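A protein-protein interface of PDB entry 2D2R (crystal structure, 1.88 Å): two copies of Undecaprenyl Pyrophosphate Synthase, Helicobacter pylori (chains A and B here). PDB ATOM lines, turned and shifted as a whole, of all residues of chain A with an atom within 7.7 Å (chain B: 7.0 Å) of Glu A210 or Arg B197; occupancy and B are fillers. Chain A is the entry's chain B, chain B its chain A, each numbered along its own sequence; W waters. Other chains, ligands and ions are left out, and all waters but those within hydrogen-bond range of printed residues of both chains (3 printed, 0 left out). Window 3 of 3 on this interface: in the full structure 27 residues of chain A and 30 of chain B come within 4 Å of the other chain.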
ATOM      1  N   HIS A  18       0.790   0.849 -31.069  1.00  0.00           N
ATOM      2  CA  HIS A  18       1.427   0.232 -29.911  1.00  0.00           C
ATOM      3  C   HIS A  18       0.421   0.150 -28.757  1.00  0.00           C
ATOM      4  O   HIS A  18       0.004   1.158 -28.195  1.00  0.00           O
ATOM      5  CB  HIS A  18       2.698   1.047 -29.543  1.00  0.00           C
ATOM      6  CG  HIS A  18       3.538   0.459 -28.437  1.00  0.00           C
ATOM      7  ND1 HIS A  18       4.770   0.972 -28.086  1.00  0.00           N
ATOM      8  CD2 HIS A  18       3.348  -0.625 -27.656  1.00  0.00           C
ATOM      9  CE1 HIS A  18       5.314   0.219 -27.148  1.00  0.00           C
ATOM     10  NE2 HIS A  18       4.473  -0.761 -26.871  1.00  0.00           N
ATOM     11  N   LEU A  19       0.103  -1.089 -28.377  1.00  0.00           N
ATOM     12  CA  LEU A  19      -0.766  -1.361 -27.239  1.00  0.00           C
ATOM     13  C   LEU A  19       0.157  -1.880 -26.121  1.00  0.00           C
ATOM     14  O   LEU A  19       1.011  -2.704 -26.366  1.00  0.00           O
ATOM     15  CB  LEU A  19      -1.788  -2.473 -27.614  1.00  0.00           C
ATOM     16  CG  LEU A  19      -2.638  -3.095 -26.477  1.00  0.00           C
ATOM     17  CD1 LEU A  19      -3.472  -1.953 -25.859  1.00  0.00           C
ATOM     18  CD2 LEU A  19      -3.622  -4.161 -27.040  1.00  0.00           C
ATOM     19  N   ALA A  20      -0.019  -1.395 -24.898  1.00  0.00           N
ATOM     20  CA  ALA A  20       0.741  -1.915 -23.761  1.00  0.00           C
ATOM     21  C   ALA A  20      -0.284  -2.367 -22.712  1.00  0.00           C
ATOM     22  O   ALA A  20      -1.341  -1.722 -22.507  1.00  0.00           O
ATOM     23  CB  ALA A  20       1.683  -0.841 -23.189  1.00  0.00           C
ATOM     24  N   VAL A 186       3.638   4.513 -27.015  1.00  0.00           N
ATOM     25  CA  VAL A 186       2.453   3.761 -26.644  1.00  0.00           C
ATOM     26  C   VAL A 186       1.185   4.533 -26.991  1.00  0.00           C
ATOM     27  O   VAL A 186       1.014   5.679 -26.575  1.00  0.00           O
ATOM     28  CB  VAL A 186       2.474   3.517 -25.146  1.00  0.00           C
ATOM     29  CG1 VAL A 186       1.134   2.733 -24.725  1.00  0.00           C
ATOM     30  CG2 VAL A 186       3.649   2.659 -24.773  1.00  0.00           C
ATOM     31  N   ASP A 187       0.254   3.932 -27.700  1.00  0.00           N
ATOM     32  CA  ASP A 187      -0.971   4.646 -28.025  1.00  0.00           C
ATOM     33  C   ASP A 187      -2.051   4.385 -26.997  1.00  0.00           C
ATOM     34  O   ASP A 187      -2.885   5.225 -26.721  1.00  0.00           O
ATOM     35  CB  ASP A 187      -1.527   4.160 -29.351  1.00  0.00           C
ATOM     36  CG  ASP A 187      -0.616   4.457 -30.496  1.00  0.00           C
ATOM     37  OD1 ASP A 187      -0.418   5.646 -30.733  1.00  0.00           O
ATOM     38  OD2 ASP A 187      -0.090   3.546 -31.145  1.00  0.00           O
ATOM     39  N   LEU A 188      -2.057   3.172 -26.453  1.00  0.00           N
ATOM     40  CA  LEU A 188      -3.089   2.809 -25.508  1.00  0.00           C
ATOM     41  C   LEU A 188      -2.428   1.989 -24.408  1.00  0.00           C
ATOM     42  O   LEU A 188      -1.766   1.000 -24.761  1.00  0.00           O
ATOM     43  CB  LEU A 188      -4.127   1.924 -26.250  1.00  0.00           C
ATOM     44  CG  LEU A 188      -5.476   1.640 -25.623  1.00  0.00           C
ATOM     45  CD1 LEU A 188      -6.337   0.845 -26.637  1.00  0.00           C
ATOM     46  CD2 LEU A 188      -5.348   0.819 -24.293  1.00  0.00           C
ATOM     47  N   LEU A 189      -2.560   2.407 -23.136  1.00  0.00           N
ATOM     48  CA  LEU A 189      -1.962   1.610 -22.015  1.00  0.00           C
ATOM     49  C   LEU A 189      -3.192   1.075 -21.216  1.00  0.00           C
ATOM     50  O   LEU A 189      -3.985   1.863 -20.736  1.00  0.00           O
ATOM     51  CB  LEU A 189      -1.095   2.527 -21.110  1.00  0.00           C
ATOM     52  CG  LEU A 189      -0.629   1.894 -19.775  1.00  0.00           C
ATOM     53  CD1 LEU A 189       0.163   0.637 -20.006  1.00  0.00           C
ATOM     54  CD2 LEU A 189       0.289   2.915 -19.059  1.00  0.00           C
ATOM     55  N   LEU A 190      -3.352  -0.251 -21.154  1.00  0.00           N
ATOM     56  CA  LEU A 190      -4.471  -0.861 -20.484  1.00  0.00           C
ATOM     57  C   LEU A 190      -4.014  -1.650 -19.255  1.00  0.00           C
ATOM     58  O   LEU A 190      -2.971  -2.312 -19.293  1.00  0.00           O
ATOM     59  CB  LEU A 190      -5.158  -1.850 -21.488  1.00  0.00           C
ATOM     60  CG  LEU A 190      -5.954  -2.997 -20.883  1.00  0.00           C
ATOM     61  CD1 LEU A 190      -7.304  -2.384 -20.382  1.00  0.00           C
ATOM     62  CD2 LEU A 190      -6.243  -4.079 -21.927  1.00  0.00           C
ATOM     63  N   SER A 206       4.483   6.265 -22.442  1.00  0.00           N
ATOM     64  CA  SER A 206       3.008   6.393 -22.388  1.00  0.00           C
ATOM     65  C   SER A 206       2.595   7.823 -22.116  1.00  0.00           C
ATOM     66  O   SER A 206       1.475   8.051 -21.697  1.00  0.00           O
ATOM     67  CB  SER A 206       2.455   5.512 -21.258  1.00  0.00           C
ATOM     68  OG  SER A 206       2.894   4.160 -21.444  1.00  0.00           O
ATOM     69  N   SER A 207       3.515   8.779 -22.302  1.00  0.00           N
ATOM     70  CA  SER A 207       3.203  10.188 -21.994  1.00  0.00           C
ATOM     71  C   SER A 207       1.842  10.736 -22.489  1.00  0.00           C
ATOM     72  O   SER A 207       1.193  11.595 -21.786  1.00  0.00           O
ATOM     73  CB  SER A 207       4.308  11.090 -22.552  1.00  0.00           C
ATOM     74  OG  SER A 207       4.061  12.365 -21.971  1.00  0.00           O
ATOM     75  N   TYR A 208       1.433  10.318 -23.699  1.00  0.00           N
ATOM     76  CA  TYR A 208       0.174  10.776 -24.271  1.00  0.00           C
ATOM     77  C   TYR A 208      -0.712   9.573 -24.648  1.00  0.00           C
ATOM     78  O   TYR A 208      -1.651   9.693 -25.422  1.00  0.00           O
ATOM     79  CB  TYR A 208       0.374  11.643 -25.539  1.00  0.00           C
ATOM     80  CG  TYR A 208       1.050  12.977 -25.253  1.00  0.00           C
ATOM     81  CD1 TYR A 208       0.337  14.036 -24.694  1.00  0.00           C
ATOM     82  CD2 TYR A 208       2.399  13.147 -25.487  1.00  0.00           C
ATOM     83  CE1 TYR A 208       0.978  15.227 -24.379  1.00  0.00           C
ATOM     84  CE2 TYR A 208       3.031  14.310 -25.167  1.00  0.00           C
ATOM     85  CZ  TYR A 208       2.323  15.341 -24.615  1.00  0.00           C
ATOM     86  OH  TYR A 208       3.006  16.491 -24.285  1.00  0.00           O
ATOM     87  N   ALA A 209      -0.474   8.445 -24.022  1.00  0.00           N
ATOM     88  CA  ALA A 209      -1.293   7.245 -24.303  1.00  0.00           C
ATOM     89  C   ALA A 209      -2.720   7.398 -23.729  1.00  0.00           C
ATOM     90  O   ALA A 209      -2.926   7.990 -22.669  1.00  0.00           O
ATOM     91  CB  ALA A 209      -0.633   6.002 -23.615  1.00  0.00           C
ATOM     92  N   GLU A 210      -3.702   6.804 -24.377  1.00  0.00           N
ATOM     93  CA  GLU A 210      -5.060   6.792 -23.850  1.00  0.00           C
ATOM     94  C   GLU A 210      -5.001   5.701 -22.796  1.00  0.00           C
ATOM     95  O   GLU A 210      -4.484   4.595 -23.116  1.00  0.00           O
ATOM     96  CB  GLU A 210      -6.059   6.338 -24.938  1.00  0.00           C
ATOM     97  CG  GLU A 210      -6.304   7.418 -25.962  1.00  0.00           C
ATOM     98  CD  GLU A 210      -7.005   8.667 -25.344  1.00  0.00           C
ATOM     99  OE1 GLU A 210      -6.873   9.769 -25.910  1.00  0.00           O
ATOM    100  OE2 GLU A 210      -7.716   8.542 -24.314  1.00  0.00           O
ATOM    101  N   LEU A 211      -5.514   5.977 -21.578  1.00  0.00           N
ATOM    102  CA  LEU A 211      -5.481   4.981 -20.501  1.00  0.00           C
ATOM    103  C   LEU A 211      -6.801   4.268 -20.386  1.00  0.00           C
ATOM    104  O   LEU A 211      -7.822   4.909 -20.442  1.00  0.00           O
ATOM    105  CB  LEU A 211      -5.155   5.633 -19.126  1.00  0.00           C
ATOM    106  CG  LEU A 211      -3.881   6.515 -19.120  1.00  0.00           C
ATOM    107  CD1 LEU A 211      -3.832   7.389 -17.890  1.00  0.00           C
ATOM    108  CD2 LEU A 211      -2.688   5.681 -19.274  1.00  0.00           C
ATOM    109  N   PHE A 212      -6.753   2.935 -20.220  1.00  0.00           N
ATOM    110  CA  PHE A 212      -7.920   2.089 -20.032  1.00  0.00           C
ATOM    111  C   PHE A 212      -7.682   1.215 -18.848  1.00  0.00           C
ATOM    112  O   PHE A 212      -6.581   0.745 -18.633  1.00  0.00           O
ATOM    113  CB  PHE A 212      -8.208   1.197 -21.271  1.00  0.00           C
ATOM    114  CG  PHE A 212      -8.924   1.967 -22.405  1.00  0.00           C
ATOM    115  CD1 PHE A 212      -8.168   2.753 -23.296  1.00  0.00           C
ATOM    116  CD2 PHE A 212     -10.320   1.897 -22.567  1.00  0.00           C
ATOM    117  CE1 PHE A 212      -8.802   3.448 -24.357  1.00  0.00           C
ATOM    118  CE2 PHE A 212     -10.974   2.584 -23.618  1.00  0.00           C
ATOM    119  CZ  PHE A 212     -10.191   3.362 -24.516  1.00  0.00           C
ATOM    120  N   PHE A 213      -8.765   0.940 -18.123  1.00  0.00           N
ATOM    121  CA  PHE A 213      -8.699   0.094 -16.954  1.00  0.00           C
ATOM    122  C   PHE A 213      -9.874  -0.864 -16.970  1.00  0.00           C
ATOM    123  O   PHE A 213     -10.986  -0.480 -17.354  1.00  0.00           O
ATOM    124  CB  PHE A 213      -8.826   0.972 -15.685  1.00  0.00           C
ATOM    125  CG  PHE A 213      -7.782   2.037 -15.590  1.00  0.00           C
ATOM    126  CD1 PHE A 213      -6.540   1.734 -15.103  1.00  0.00           C
ATOM    127  CD2 PHE A 213      -8.018   3.307 -16.100  1.00  0.00           C
ATOM    128  CE1 PHE A 213      -5.534   2.664 -15.153  1.00  0.00           C
ATOM    129  CE2 PHE A 213      -7.023   4.254 -16.146  1.00  0.00           C
ATOM    130  CZ  PHE A 213      -5.803   3.955 -15.699  1.00  0.00           C
ATOM    131  N   ASP A 232     -13.624   1.333 -28.226  1.00  0.00           N
ATOM    132  CA  ASP A 232     -13.708   2.518 -27.325  1.00  0.00           C
ATOM    133  C   ASP A 232     -12.584   3.497 -27.556  1.00  0.00           C
ATOM    134  O   ASP A 232     -12.784   4.736 -27.489  1.00  0.00           O
ATOM    135  CB  ASP A 232     -13.693   2.101 -25.891  1.00  0.00           C
ATOM    136  CG  ASP A 232     -15.074   1.650 -25.421  1.00  0.00           C
ATOM    137  OD1 ASP A 232     -15.180   1.132 -24.287  1.00  0.00           O
ATOM    138  OD2 ASP A 232     -16.030   1.838 -26.217  1.00  0.00           O
ATOM    139  N   PHE A 233     -11.409   2.970 -27.819  1.00  0.00           N
ATOM    140  CA  PHE A 233     -10.234   3.790 -28.105  1.00  0.00           C
ATOM    141  C   PHE A 233     -10.526   4.671 -29.350  1.00  0.00           C
ATOM    142  O   PHE A 233     -10.356   5.896 -29.351  1.00  0.00           O
ATOM    143  CB  PHE A 233      -9.057   2.890 -28.424  1.00  0.00           C
ATOM    144  CG  PHE A 233      -7.868   3.627 -28.978  1.00  0.00           C
ATOM    145  CD1 PHE A 233      -6.967   4.258 -28.132  1.00  0.00           C
ATOM    146  CD2 PHE A 233      -7.641   3.669 -30.356  1.00  0.00           C
ATOM    147  CE1 PHE A 233      -5.858   4.921 -28.638  1.00  0.00           C
ATOM    148  CE2 PHE A 233      -6.510   4.354 -30.882  1.00  0.00           C
ATOM    149  CZ  PHE A 233      -5.633   4.969 -30.032  1.00  0.00           C
ATOM    150  N   TYR A 234     -10.949   4.038 -30.434  1.00  0.00           N
ATOM    151  CA  TYR A 234     -11.269   4.785 -31.641  1.00  0.00           C
ATOM    152  C   TYR A 234     -12.384   5.780 -31.413  1.00  0.00           C
ATOM    153  O   TYR A 234     -12.373   6.866 -32.019  1.00  0.00           O
ATOM    154  CB  TYR A 234     -11.603   3.842 -32.777  1.00  0.00           C
ATOM    155  CG  TYR A 234     -10.327   3.254 -33.349  1.00  0.00           C
ATOM    156  CD1 TYR A 234      -9.419   4.056 -34.021  1.00  0.00           C
ATOM    157  CD2 TYR A 234     -10.017   1.909 -33.175  1.00  0.00           C
ATOM    158  CE1 TYR A 234      -8.211   3.506 -34.548  1.00  0.00           C
ATOM    159  CE2 TYR A 234      -8.834   1.376 -33.654  1.00  0.00           C
ATOM    160  CZ  TYR A 234      -7.934   2.189 -34.342  1.00  0.00           C
ATOM    161  OH  TYR A 234      -6.741   1.653 -34.832  1.00  0.00           O
ATOM    162  N   ARG A 236     -12.880   7.346 -28.585  1.00  0.00           N
ATOM    163  CA  ARG A 236     -12.278   8.510 -27.879  1.00  0.00           C
ATOM    164  C   ARG A 236     -11.559   9.395 -28.887  1.00  0.00           C
ATOM    165  O   ARG A 236     -11.602  10.661 -28.840  1.00  0.00           O
ATOM    166  CB  ARG A 236     -11.230   8.056 -26.851  1.00  0.00           C
ATOM    167  CG  ARG A 236     -11.776   7.231 -25.714  1.00  0.00           C
ATOM    168  CD  ARG A 236     -10.639   7.104 -24.690  1.00  0.00           C
ATOM    169  NE  ARG A 236     -10.971   6.316 -23.519  1.00  0.00           N
ATOM    170  CZ  ARG A 236     -10.102   6.089 -22.540  1.00  0.00           C
ATOM    171  NH1 ARG A 236      -8.858   6.614 -22.598  1.00  0.00           N
ATOM    172  NH2 ARG A 236     -10.437   5.285 -21.538  1.00  0.00           N
ATOM    173  N   VAL A 237     -10.867   8.766 -29.808  1.00  0.00           N
ATOM    174  CA  VAL A 237     -10.124   9.535 -30.783  1.00  0.00           C
ATOM    175  C   VAL A 237     -11.029  10.430 -31.652  1.00  0.00           C
ATOM    176  O   VAL A 237     -10.626  11.526 -32.047  1.00  0.00           O
ATOM    177  CB  VAL A 237      -9.259   8.624 -31.677  1.00  0.00           C
ATOM    178  CG1 VAL A 237      -8.500   9.497 -32.694  1.00  0.00           C
ATOM    179  CG2 VAL A 237      -8.297   7.790 -30.811  1.00  0.00           C
ATOM    180  N   PHE A 240     -12.330  13.626 -29.284  1.00  0.00           N
ATOM    181  CA  PHE A 240     -11.533  14.800 -28.949  1.00  0.00           C
ATOM    182  C   PHE A 240     -11.515  15.795 -30.129  1.00  0.00           C
ATOM    183  O   PHE A 240     -11.498  17.024 -29.929  1.00  0.00           O
ATOM    184  CB  PHE A 240     -10.118  14.396 -28.511  1.00  0.00           C
ATOM    185  CG  PHE A 240      -9.251  13.934 -29.623  1.00  0.00           C
ATOM    186  CD1 PHE A 240      -8.702  14.847 -30.514  1.00  0.00           C
ATOM    187  CD2 PHE A 240      -8.972  12.584 -29.781  1.00  0.00           C
ATOM    188  CE1 PHE A 240      -7.881  14.425 -31.557  1.00  0.00           C
ATOM    189  CE2 PHE A 240      -8.155  12.149 -30.819  1.00  0.00           C
ATOM    190  CZ  PHE A 240      -7.607  13.072 -31.710  1.00  0.00           C
ATOM    191  N   ILE B  22      -4.699  17.642 -13.060  1.00  0.00           N
ATOM    192  CA  ILE B  22      -4.668  18.171 -14.437  1.00  0.00           C
ATOM    193  C   ILE B  22      -6.066  18.863 -14.468  1.00  0.00           C
ATOM    194  O   ILE B  22      -7.111  18.214 -14.424  1.00  0.00           O
ATOM    195  CB  ILE B  22      -4.561  17.000 -15.484  1.00  0.00           C
ATOM    196  CG1 ILE B  22      -3.133  16.410 -15.379  1.00  0.00           C
ATOM    197  CG2 ILE B  22      -4.842  17.508 -16.913  1.00  0.00           C
ATOM    198  CD1 ILE B  22      -2.971  15.040 -15.930  1.00  0.00           C
ATOM    199  N   ASP B  24      -8.546  20.157 -16.362  1.00  0.00           N
ATOM    200  CA  ASP B  24      -9.043  20.283 -17.707  1.00  0.00           C
ATOM    201  C   ASP B  24     -10.556  20.632 -17.760  1.00  0.00           C
ATOM    202  O   ASP B  24     -11.282  20.465 -16.777  1.00  0.00           O
ATOM    203  CB  ASP B  24      -8.733  18.971 -18.436  1.00  0.00           C
ATOM    204  CG  ASP B  24      -8.827  19.091 -19.938  1.00  0.00           C
ATOM    205  OD1 ASP B  24      -8.479  20.183 -20.468  1.00  0.00           O
ATOM    206  OD2 ASP B  24      -9.240  18.091 -20.596  1.00  0.00           O
ATOM    207  N   LEU B 189      -3.201  11.230  -8.572  1.00  0.00           N
ATOM    208  CA  LEU B 189      -3.139  12.139  -9.731  1.00  0.00           C
ATOM    209  C   LEU B 189      -4.546  12.179 -10.293  1.00  0.00           C
ATOM    210  O   LEU B 189      -5.109  11.163 -10.699  1.00  0.00           O
ATOM    211  CB  LEU B 189      -2.146  11.610 -10.797  1.00  0.00           C
ATOM    212  CG  LEU B 189      -2.173  12.403 -12.106  1.00  0.00           C
ATOM    213  CD1 LEU B 189      -1.782  13.875 -11.819  1.00  0.00           C
ATOM    214  CD2 LEU B 189      -1.206  11.820 -13.084  1.00  0.00           C
ATOM    215  N   ARG B 191      -7.463  13.876 -12.883  1.00  0.00           N
ATOM    216  CA  ARG B 191      -7.663  14.649 -14.117  1.00  0.00           C
ATOM    217  C   ARG B 191      -9.156  14.914 -14.299  1.00  0.00           C
ATOM    218  O   ARG B 191      -9.980  13.991 -14.341  1.00  0.00           O
ATOM    219  CB  ARG B 191      -7.104  13.940 -15.374  1.00  0.00           C
ATOM    220  CG  ARG B 191      -7.425  14.697 -16.651  1.00  0.00           C
ATOM    221  CD  ARG B 191      -6.567  14.324 -17.837  1.00  0.00           C
ATOM    222  NE  ARG B 191      -6.884  15.167 -18.977  1.00  0.00           N
ATOM    223  CZ  ARG B 191      -6.087  15.337 -20.014  1.00  0.00           C
ATOM    224  NH1 ARG B 191      -4.915  14.668 -20.043  1.00  0.00           N
ATOM    225  NH2 ARG B 191      -6.401  16.238 -20.965  1.00  0.00           N
ATOM    226  N   GLY B 194     -12.977  14.839 -18.249  1.00  0.00           N
ATOM    227  CA  GLY B 194     -13.368  13.762 -19.145  1.00  0.00           C
ATOM    228  C   GLY B 194     -12.324  12.913 -19.870  1.00  0.00           C
ATOM    229  O   GLY B 194     -12.610  11.759 -20.198  1.00  0.00           O
ATOM    230  N   GLU B 195     -11.149  13.475 -20.140  1.00  0.00           N
ATOM    231  CA  GLU B 195     -10.082  12.755 -20.853  1.00  0.00           C
ATOM    232  C   GLU B 195      -9.354  11.817 -19.934  1.00  0.00           C
ATOM    233  O   GLU B 195      -9.275  12.040 -18.742  1.00  0.00           O
ATOM    234  CB  GLU B 195      -9.064  13.714 -21.447  1.00  0.00           C
ATOM    235  CG  GLU B 195      -9.598  14.647 -22.529  1.00  0.00           C
ATOM    236  CD  GLU B 195     -10.380  13.936 -23.628  1.00  0.00           C
ATOM    237  OE1 GLU B 195     -10.019  12.825 -24.058  1.00  0.00           O
ATOM    238  OE2 GLU B 195     -11.366  14.505 -24.096  1.00  0.00           O
ATOM    239  N   MET B 196      -8.791  10.748 -20.503  1.00  0.00           N
ATOM    240  CA  MET B 196      -8.045   9.796 -19.667  1.00  0.00           C
ATOM    241  C   MET B 196      -6.652   9.591 -20.249  1.00  0.00           C
ATOM    242  O   MET B 196      -6.404   8.584 -20.869  1.00  0.00           O
ATOM    243  CB  MET B 196      -8.824   8.486 -19.597  1.00  0.00           C
ATOM    244  CG  MET B 196     -10.077   8.701 -18.753  1.00  0.00           C
ATOM    245  SD  MET B 196     -11.209   7.285 -18.720  1.00  0.00           S
ATOM    246  CE  MET B 196     -10.180   5.977 -17.885  1.00  0.00           C
ATOM    247  N   ARG B 197      -5.760  10.550 -20.025  1.00  0.00           N
ATOM    248  CA  ARG B 197      -4.363  10.513 -20.570  1.00  0.00           C
ATOM    249  C   ARG B 197      -3.529  11.253 -19.530  1.00  0.00           C
ATOM    250  O   ARG B 197      -4.095  12.124 -18.863  1.00  0.00           O
ATOM    251  CB  ARG B 197      -4.277  11.341 -21.873  1.00  0.00           C
ATOM    252  CG  ARG B 197      -4.830  10.675 -23.148  1.00  0.00           C
ATOM    253  CD  ARG B 197      -4.408  11.480 -24.425  1.00  0.00           C
ATOM    254  NE  ARG B 197      -4.878  12.852 -24.352  1.00  0.00           N
ATOM    255  CZ  ARG B 197      -6.147  13.210 -24.526  1.00  0.00           C
ATOM    256  NH1 ARG B 197      -7.072  12.293 -24.809  1.00  0.00           N
ATOM    257  NH2 ARG B 197      -6.502  14.479 -24.385  1.00  0.00           N
ATOM    258  N   LEU B 198      -2.209  10.987 -19.426  1.00  0.00           N
ATOM    259  CA  LEU B 198      -1.382  11.695 -18.418  1.00  0.00           C
ATOM    260  C   LEU B 198      -0.930  13.051 -18.960  1.00  0.00           C
ATOM    261  O   LEU B 198      -0.576  13.965 -18.198  1.00  0.00           O
ATOM    262  CB  LEU B 198      -0.105  10.931 -18.103  1.00  0.00           C
ATOM    263  CG  LEU B 198      -0.423   9.524 -17.675  1.00  0.00           C
ATOM    264  CD1 LEU B 198       0.891   8.686 -17.764  1.00  0.00           C
ATOM    265  CD2 LEU B 198      -0.952   9.567 -16.273  1.00  0.00           C
ATOM    266  N   SER B 199      -0.903  13.141 -20.281  1.00  0.00           N
ATOM    267  CA  SER B 199      -0.463  14.353 -20.930  1.00  0.00           C
ATOM    268  C   SER B 199       0.888  14.891 -20.496  1.00  0.00           C
ATOM    269  O   SER B 199       1.018  16.096 -20.227  1.00  0.00           O
ATOM    270  CB  SER B 199      -1.552  15.430 -20.773  1.00  0.00           C
ATOM    271  OG  SER B 199      -2.610  15.089 -21.671  1.00  0.00           O
ATOM    272  N   ASN B 200       1.892  14.019 -20.429  1.00  0.00           N
ATOM    273  CA  ASN B 200       3.282  14.450 -20.143  1.00  0.00           C
ATOM    274  C   ASN B 200       3.408  15.271 -18.839  1.00  0.00           C
ATOM    275  O   ASN B 200       4.131  16.242 -18.769  1.00  0.00           O
ATOM    276  CB  ASN B 200       3.721  15.260 -21.361  1.00  0.00           C
ATOM    277  CG  ASN B 200       5.203  15.460 -21.441  1.00  0.00           C
ATOM    278  OD1 ASN B 200       5.997  14.662 -20.957  1.00  0.00           O
ATOM    279  ND2 ASN B 200       5.600  16.588 -22.042  1.00  0.00           N
ATOM    280  N   PHE B 213     -10.148   9.926 -12.424  1.00  0.00           N
ATOM    281  CA  PHE B 213     -10.663  10.641 -13.575  1.00  0.00           C
ATOM    282  C   PHE B 213     -12.128  11.061 -13.323  1.00  0.00           C
ATOM    283  O   PHE B 213     -12.890  10.349 -12.683  1.00  0.00           O
ATOM    284  CB  PHE B 213     -10.601   9.708 -14.816  1.00  0.00           C
ATOM    285  CG  PHE B 213      -9.214   9.264 -15.138  1.00  0.00           C
ATOM    286  CD1 PHE B 213      -8.329  10.095 -15.823  1.00  0.00           C
ATOM    287  CD2 PHE B 213      -8.750   8.054 -14.664  1.00  0.00           C
ATOM    288  CE1 PHE B 213      -6.991   9.729 -16.036  1.00  0.00           C
ATOM    289  CE2 PHE B 213      -7.433   7.687 -14.860  1.00  0.00           C
ATOM    290  CZ  PHE B 213      -6.561   8.525 -15.545  1.00  0.00           C
HETATM  291  O   HOH W   1      -9.297  10.353 -23.272  1.00  0.00           O
HETATM  292  O   HOH W   2      -1.279   9.022 -20.826  1.00  0.00           O
HETATM  293  O   HOH W   3       3.451  19.138 -22.204  1.00  0.00           O
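C of Leu B198 touches O of Ser A207 (3.8 Å). CD of Arg B197 touches O of Tyr A208, 3.4 Å away. CA of Ser B199 touches CE1 of Tyr A208, 3.8 Å away. Ala A209 touches Met B196. O of Ala A209 touches CG of Arg B197, 3.3 Å away. Met B196 touches Glu A210. Leu B198 touches Leu A211. Phe B213 touches Leu A211 (CZ to CD1, 3.8 Å). Phe A213 touches Met B196 (CD2 to CE, 3.9 Å). Phe B213 touches Phe A213.
Phe B213 touches its own counterpart, Phe A213. 2 positions are printed for both chains.
The guanidinium group (NH1) of Arg B191 lies within hydrogen-bond range of the backbone carbonyl oxygen (O) of Arg B197, 2.9 Å away. The side-chain hydroxyl (OG) of Ser B199 sits at hydrogen-bond distance from the guanidinium group (NH1) of Arg B191 (2.9 Å). The guanidinium group of Arg B197 is in salt-bridge range of the side-chain carboxylate of Glu B195 (3.1 Å). The backbone NH (N) of Leu A189 lies within hydrogen-bond range of the backbone carbonyl oxygen (O) of Glu A210 (2.9 Å). OE2 of Glu A210 is in salt-bridge range of NH1 of Arg A236, 2.8 Å away. O of Leu A211 lies within hydrogen-bond range of NH2 of Arg A236, 2.9 Å away.
Glu A210 touches two residues of chain B. Arg B197 touches three residues of chain A. Printed residues of chain A within 4 Å of Ser B199: Ser A207 (3.0 Å) and Tyr A208 (3.8 Å). Printed residues of chain B within 4 Å of Leu A211: Met B196 (2.8 Å), Leu B198 (3.96 Å) and Phe B213 (3.8 Å). Of the printed residues of chain B, Tyr A208 touches Arg B197, Ser B199 and Asn B200.
The backbone NH of Leu A211 is in hydrogen-bond range of the backbone carbonyl oxygen of Met B196, at 2.8 Å. The side-chain sulfur of Met B196 sits at hydrogen-bond distance from the guanidinium group of Arg A236. NH1 of Arg B197 lies within salt-bridge range of OE1 of Glu A210, at 2.8 Å. The backbone carbonyl oxygen of Ser A207 lies within hydrogen-bond range of the backbone NH of Ser B199. The backbone NH (N) of Asn B200 sits at hydrogen-bond distance from the backbone carbonyl oxygen (O) of Ser A207, at 2.9 Å. OH of Tyr A208 sits close to ND2 of Asn B200.
Of the 12 printed residues of chain B, 6 touch a printed residue of chain A. Hydrophobic or aromatic side chains of chain B within 4 Å of the printed part of chain A: Met B196, Leu B198 and Phe B213. Of the 22 printed residues of chain A, 7 touch a printed residue of chain B. Along chain A the printed residues that touch a printed residue of chain B span positions 207 to 236.
Water W2 lies within hydrogen-bond range of N of Leu B198 (2.6 Å), O of Ala A209 (2.7 Å) and O of Ser A206 (3.0 Å). Water W1 lies within hydrogen-bond range of OE2 of Glu A210 (2.6 Å), OE1 of Glu B195 (2.7 Å), N of Met B196 (2.8 Å) and NH1 of Arg B197 (3.3 Å). Water W3 bridges ND2 of Asn B200 (3.3 Å) and OH of Tyr A208 (3.4 Å).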
